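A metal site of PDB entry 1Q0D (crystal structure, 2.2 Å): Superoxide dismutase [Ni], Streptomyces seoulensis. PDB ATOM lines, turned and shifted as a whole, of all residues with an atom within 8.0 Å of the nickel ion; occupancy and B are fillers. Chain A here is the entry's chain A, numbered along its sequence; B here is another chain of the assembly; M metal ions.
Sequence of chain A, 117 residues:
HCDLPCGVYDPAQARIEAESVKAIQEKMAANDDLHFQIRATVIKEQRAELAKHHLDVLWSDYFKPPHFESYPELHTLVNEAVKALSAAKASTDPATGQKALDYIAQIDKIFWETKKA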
ATOM      1  N   HIS A   1     -10.861  22.023   7.299  1.00  0.00           N
ATOM      2  CA  HIS A   1      -9.646  21.174   7.160  1.00  0.00           C
ATOM      3  C   HIS A   1      -9.069  21.205   5.729  1.00  0.00           C
ATOM      4  O   HIS A   1      -7.919  20.853   5.504  1.00  0.00           O
ATOM      5  CB  HIS A   1      -9.979  19.733   7.618  1.00  0.00           C
ATOM      6  CG  HIS A   1     -10.887  18.969   6.694  1.00  0.00           C
ATOM      7  ND1 HIS A   1     -11.625  19.559   5.701  1.00  0.00           N
ATOM      8  CD2 HIS A   1     -11.170  17.640   6.637  1.00  0.00           C
ATOM      9  CE1 HIS A   1     -12.314  18.638   5.065  1.00  0.00           C
ATOM     10  NE2 HIS A   1     -12.066  17.465   5.612  1.00  0.00           N
ATOM     11  N   CYS A   2      -9.892  21.699   4.797  1.00  0.00           N
ATOM     12  CA  CYS A   2      -9.550  21.834   3.370  1.00  0.00           C
ATOM     13  C   CYS A   2      -8.976  23.224   3.004  1.00  0.00           C
ATOM     14  O   CYS A   2      -8.708  23.493   1.837  1.00  0.00           O
ATOM     15  CB  CYS A   2     -10.795  21.535   2.550  1.00  0.00           C
ATOM     16  SG  CYS A   2     -12.118  22.565   3.130  1.00  0.00           S
ATOM     17  N   ASP A   3      -8.908  24.116   3.972  1.00  0.00           N
ATOM     18  CA  ASP A   3      -8.336  25.467   3.769  1.00  0.00           C
ATOM     19  C   ASP A   3      -9.188  26.458   2.967  1.00  0.00           C
ATOM     20  O   ASP A   3      -8.668  27.487   2.511  1.00  0.00           O
ATOM     21  CB  ASP A   3      -6.961  25.323   3.069  1.00  0.00           C
ATOM     22  CG  ASP A   3      -5.898  26.259   3.643  1.00  0.00           C
ATOM     23  OD1 ASP A   3      -6.226  27.077   4.521  1.00  0.00           O
ATOM     24  OD2 ASP A   3      -4.730  26.173   3.205  1.00  0.00           O
ATOM     25  N   LEU A   4     -10.474  26.176   2.796  1.00  0.00           N
ATOM     26  CA  LEU A   4     -11.347  27.081   2.047  1.00  0.00           C
ATOM     27  C   LEU A   4     -11.460  28.466   2.700  1.00  0.00           C
ATOM     28  O   LEU A   4     -11.296  29.478   2.020  1.00  0.00           O
ATOM     29  CB  LEU A   4     -12.749  26.497   1.889  1.00  0.00           C
ATOM     30  CG  LEU A   4     -13.753  27.440   1.209  1.00  0.00           C
ATOM     31  CD1 LEU A   4     -13.219  27.879  -0.157  1.00  0.00           C
ATOM     32  CD2 LEU A   4     -15.096  26.739   1.051  1.00  0.00           C
ATOM     33  N   PRO A   5     -11.736  28.533   4.012  1.00  0.00           N
ATOM     34  CA  PRO A   5     -11.958  27.450   4.986  1.00  0.00           C
ATOM     35  C   PRO A   5     -13.388  26.906   4.959  1.00  0.00           C
ATOM     36  O   PRO A   5     -14.321  27.608   4.550  1.00  0.00           O
ATOM     37  CB  PRO A   5     -11.615  28.106   6.312  1.00  0.00           C
ATOM     38  CG  PRO A   5     -12.208  29.482   6.115  1.00  0.00           C
ATOM     39  CD  PRO A   5     -11.766  29.843   4.690  1.00  0.00           C
ATOM     40  N   CYS A   6     -13.566  25.666   5.403  1.00  0.00           N
ATOM     41  CA  CYS A   6     -14.878  25.037   5.423  1.00  0.00           C
ATOM     42  C   CYS A   6     -15.465  24.968   6.835  1.00  0.00           C
ATOM     43  O   CYS A   6     -16.657  24.719   7.006  1.00  0.00           O
ATOM     44  CB  CYS A   6     -14.807  23.630   4.838  1.00  0.00           C
ATOM     45  SG  CYS A   6     -13.866  22.458   5.850  1.00  0.00           S
ATOM     46  N   GLY A   7     -14.614  25.175   7.842  1.00  0.00           N
ATOM     47  CA  GLY A   7     -15.072  25.147   9.217  1.00  0.00           C
ATOM     48  C   GLY A   7     -15.292  23.760   9.804  1.00  0.00           C
ATOM     49  O   GLY A   7     -15.815  23.632  10.910  1.00  0.00           O
ATOM     50  N   VAL A   8     -14.919  22.721   9.063  1.00  0.00           N
ATOM     51  CA  VAL A   8     -15.092  21.357   9.551  1.00  0.00           C
ATOM     52  C   VAL A   8     -13.739  20.739   9.899  1.00  0.00           C
ATOM     53  O   VAL A   8     -12.851  20.617   9.044  1.00  0.00           O
ATOM     54  CB  VAL A   8     -15.794  20.480   8.482  1.00  0.00           C
ATOM     55  CG1 VAL A   8     -15.932  19.040   8.993  1.00  0.00           C
ATOM     56  CG2 VAL A   8     -17.168  21.053   8.148  1.00  0.00           C
ATOM     57  N   TYR A   9     -13.572  20.367  11.165  1.00  0.00           N
ATOM     58  CA  TYR A   9     -12.337  19.754  11.639  1.00  0.00           C
ATOM     59  C   TYR A   9     -12.667  18.715  12.678  1.00  0.00           C
ATOM     60  O   TYR A   9     -13.671  18.833  13.384  1.00  0.00           O
ATOM     61  CB  TYR A   9     -11.423  20.763  12.297  1.00  0.00           C
ATOM     62  CG  TYR A   9     -10.904  21.878  11.441  1.00  0.00           C
ATOM     63  CD1 TYR A   9      -9.706  21.708  10.743  1.00  0.00           C
ATOM     64  CD2 TYR A   9     -11.545  23.109  11.379  1.00  0.00           C
ATOM     65  CE1 TYR A   9      -9.158  22.760  10.016  1.00  0.00           C
ATOM     66  CE2 TYR A   9     -11.004  24.164  10.644  1.00  0.00           C
ATOM     67  CZ  TYR A   9      -9.811  23.979   9.972  1.00  0.00           C
ATOM     68  OH  TYR A   9      -9.251  25.026   9.259  1.00  0.00           O
ATOM     69  N   GLN A  13      -9.663  12.247  12.375  1.00  0.00           N
ATOM     70  CA  GLN A  13      -8.976  11.886  11.138  1.00  0.00           C
ATOM     71  C   GLN A  13      -7.562  11.396  11.455  1.00  0.00           C
ATOM     72  O   GLN A  13      -7.141  10.355  10.959  1.00  0.00           O
ATOM     73  CB  GLN A  13      -8.928  13.084  10.190  1.00  0.00           C
ATOM     74  CG  GLN A  13     -10.300  13.507   9.651  1.00  0.00           C
ATOM     75  CD  GLN A  13     -10.227  14.535   8.538  1.00  0.00           C
ATOM     76  OE1 GLN A  13      -9.914  15.708   8.769  1.00  0.00           O
ATOM     77  NE2 GLN A  13     -10.515  14.095   7.314  1.00  0.00           N
ATOM     78  N   VAL A  57      -2.426  19.962   9.679  1.00  0.00           N
ATOM     79  CA  VAL A  57      -3.566  20.805   9.293  1.00  0.00           C
ATOM     80  C   VAL A  57      -4.239  21.430  10.508  1.00  0.00           C
ATOM     81  O   VAL A  57      -4.620  22.602  10.478  1.00  0.00           O
ATOM     82  CB  VAL A  57      -4.614  19.974   8.502  1.00  0.00           C
ATOM     83  CG1 VAL A  57      -5.897  20.799   8.309  1.00  0.00           C
ATOM     84  CG2 VAL A  57      -4.044  19.567   7.156  1.00  0.00           C
ATOM     85  N   ASP A  61      -4.024  25.294  10.282  1.00  0.00           N
ATOM     86  CA  ASP A  61      -5.319  25.869   9.911  1.00  0.00           C
ATOM     87  C   ASP A  61      -6.342  26.070  11.030  1.00  0.00           C
ATOM     88  O   ASP A  61      -6.942  27.136  11.143  1.00  0.00           O
ATOM     89  CB  ASP A  61      -5.969  25.008   8.817  1.00  0.00           C
ATOM     90  CG  ASP A  61      -5.138  24.945   7.545  1.00  0.00           C
ATOM     91  OD1 ASP A  61      -3.965  25.361   7.547  1.00  0.00           O
ATOM     92  OD2 ASP A  61      -5.676  24.458   6.525  1.00  0.00           O
ATOM     93  N   ILE B  16     -17.027  12.774   7.552  1.00  0.00           N
ATOM     94  CA  ILE B  16     -16.385  14.070   7.772  1.00  0.00           C
ATOM     95  C   ILE B  16     -16.177  14.821   6.442  1.00  0.00           C
ATOM     96  O   ILE B  16     -16.398  16.028   6.359  1.00  0.00           O
ATOM     97  CB  ILE B  16     -15.028  13.901   8.514  1.00  0.00           C
ATOM     98  CG1 ILE B  16     -15.276  13.216   9.860  1.00  0.00           C
ATOM     99  CG2 ILE B  16     -14.376  15.255   8.733  1.00  0.00           C
ATOM    100  CD1 ILE B  16     -14.014  12.794  10.614  1.00  0.00           C
ATOM    101  N   GLU B  17     -15.766  14.108   5.399  1.00  0.00           N
ATOM    102  CA  GLU B  17     -15.553  14.744   4.104  1.00  0.00           C
ATOM    103  C   GLU B  17     -16.886  15.200   3.517  1.00  0.00           C
ATOM    104  O   GLU B  17     -16.986  16.283   2.948  1.00  0.00           O
ATOM    105  CB  GLU B  17     -14.847  13.785   3.143  1.00  0.00           C
ATOM    106  CG  GLU B  17     -13.421  13.401   3.571  1.00  0.00           C
ATOM    107  CD  GLU B  17     -12.501  14.609   3.742  1.00  0.00           C
ATOM    108  OE1 GLU B  17     -12.895  15.736   3.381  1.00  0.00           O
ATOM    109  OE2 GLU B  17     -11.384  14.418   4.257  1.00  0.00           O
ATOM    110  N   SER B  20     -17.932  18.346   5.023  1.00  0.00           N
ATOM    111  CA  SER B  20     -17.234  19.503   4.467  1.00  0.00           C
ATOM    112  C   SER B  20     -17.901  19.908   3.169  1.00  0.00           C
ATOM    113  O   SER B  20     -18.013  21.097   2.854  1.00  0.00           O
ATOM    114  CB  SER B  20     -15.765  19.180   4.204  1.00  0.00           C
ATOM    115  OG  SER B  20     -15.047  19.202   5.416  1.00  0.00           O
ATOM    116  N   VAL B  21     -18.339  18.919   2.393  1.00  0.00           N
ATOM    117  CA  VAL B  21     -19.007  19.202   1.132  1.00  0.00           C
ATOM    118  C   VAL B  21     -20.248  20.054   1.375  1.00  0.00           C
ATOM    119  O   VAL B  21     -20.430  21.082   0.718  1.00  0.00           O
ATOM    120  CB  VAL B  21     -19.421  17.911   0.399  1.00  0.00           C
ATOM    121  CG1 VAL B  21     -20.345  18.238  -0.768  1.00  0.00           C
ATOM    122  CG2 VAL B  21     -18.172  17.173  -0.092  1.00  0.00           C
ATOM    123  N   ALA B  23     -20.995  21.830   4.071  1.00  0.00           N
ATOM    124  CA  ALA B  23     -20.587  23.099   4.679  1.00  0.00           C
ATOM    125  C   ALA B  23     -20.102  24.078   3.610  1.00  0.00           C
ATOM    126  O   ALA B  23     -20.362  25.279   3.694  1.00  0.00           O
ATOM    127  CB  ALA B  23     -19.496  22.872   5.717  1.00  0.00           C
ATOM    128  N   ILE B  24     -19.386  23.556   2.615  1.00  0.00           N
ATOM    129  CA  ILE B  24     -18.888  24.403   1.540  1.00  0.00           C
ATOM    130  C   ILE B  24     -20.046  24.955   0.708  1.00  0.00           C
ATOM    131  O   ILE B  24     -20.060  26.125   0.343  1.00  0.00           O
ATOM    132  CB  ILE B  24     -17.908  23.631   0.623  1.00  0.00           C
ATOM    133  CG1 ILE B  24     -16.627  23.281   1.402  1.00  0.00           C
ATOM    134  CG2 ILE B  24     -17.564  24.459  -0.614  1.00  0.00           C
ATOM    135  CD1 ILE B  24     -15.711  22.318   0.684  1.00  0.00           C
ATOM    136  N   LYS B  27     -21.609  27.836   2.425  1.00  0.00           N
ATOM    137  CA  LYS B  27     -20.798  29.031   2.317  1.00  0.00           C
ATOM    138  C   LYS B  27     -20.879  29.653   0.922  1.00  0.00           C
ATOM    139  O   LYS B  27     -20.808  30.863   0.774  1.00  0.00           O
ATOM    140  CB  LYS B  27     -19.335  28.707   2.654  1.00  0.00           C
ATOM    141  CG  LYS B  27     -19.119  28.338   4.098  1.00  0.00           C
ATOM    142  CD  LYS B  27     -17.669  27.976   4.365  1.00  0.00           C
ATOM    143  CE  LYS B  27     -17.436  27.712   5.847  1.00  0.00           C
ATOM    144  NZ  LYS B  27     -17.732  28.924   6.655  1.00  0.00           N
ATOM    145  N   ILE B  43     -12.339  23.017  -4.131  1.00  0.00           N
ATOM    146  CA  ILE B  43     -12.226  22.293  -2.884  1.00  0.00           C
ATOM    147  C   ILE B  43     -13.379  21.313  -2.626  1.00  0.00           C
ATOM    148  O   ILE B  43     -13.166  20.220  -2.088  1.00  0.00           O
ATOM    149  CB  ILE B  43     -12.082  23.281  -1.713  1.00  0.00           C
ATOM    150  CG1 ILE B  43     -10.803  24.097  -1.906  1.00  0.00           C
ATOM    151  CG2 ILE B  43     -12.081  22.541  -0.392  1.00  0.00           C
ATOM    152  CD1 ILE B  43     -10.587  25.219  -0.922  1.00  0.00           C
ATOM    153  N   ARG B  47     -13.031  17.273  -1.784  1.00  0.00           N
ATOM    154  CA  ARG B  47     -13.569  16.605  -0.596  1.00  0.00           C
ATOM    155  C   ARG B  47     -14.619  15.564  -0.962  1.00  0.00           C
ATOM    156  O   ARG B  47     -14.700  14.501  -0.344  1.00  0.00           O
ATOM    157  CB  ARG B  47     -14.151  17.632   0.395  1.00  0.00           C
ATOM    158  CG  ARG B  47     -13.269  18.857   0.646  1.00  0.00           C
ATOM    159  CD  ARG B  47     -11.749  18.540   0.654  1.00  0.00           C
ATOM    160  NE  ARG B  47     -11.354  17.649   1.740  1.00  0.00           N
ATOM    161  CZ  ARG B  47     -10.085  17.413   2.096  1.00  0.00           C
ATOM    162  NH1 ARG B  47      -9.087  18.005   1.445  1.00  0.00           N
ATOM    163  NH2 ARG B  47      -9.814  16.583   3.092  1.00  0.00           N
HETATM  164 NI    NI M   1     -11.706  22.198   5.292  1.00  0.00          NI
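SG of Cys 6 sits close to OG of Ser 20 of chain B.
N of Val 8 sits close to SG of Cys 6 (3.4 Å).
O of Val 8 sits close to N of His 1.
A ring nitrogen (ND1) of His 1 sits close to the side-chain hydroxyl of Ser 20 of chain B (3.5 Å).
A ring nitrogen (NE2) of His 1 sits at hydrogen-bond distance from the side-chain carboxylate (OE1) of Glu 17 of chain B.
A ring nitrogen (NE2) of His 1 is in hydrogen-bond range of the guanidinium group of Arg 47 of chain B, at 3.5 Å.
Residues that only touch the nickel ion: Asp 3.
The nickel ion is bound by the backbone nitrogen of Cys 2 (1.9 Å), the backbone nitrogen of His 1 (2.2 Å), the side-chain sulfur of Cys 2 (2.2 Å) and the side-chain sulfur of Cys 6 (2.2 Å).
The nickel ion has four donor atoms within binding distance.
Slightly farther from the nickel ion lies ND1 of His 1 (2.7 Å).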
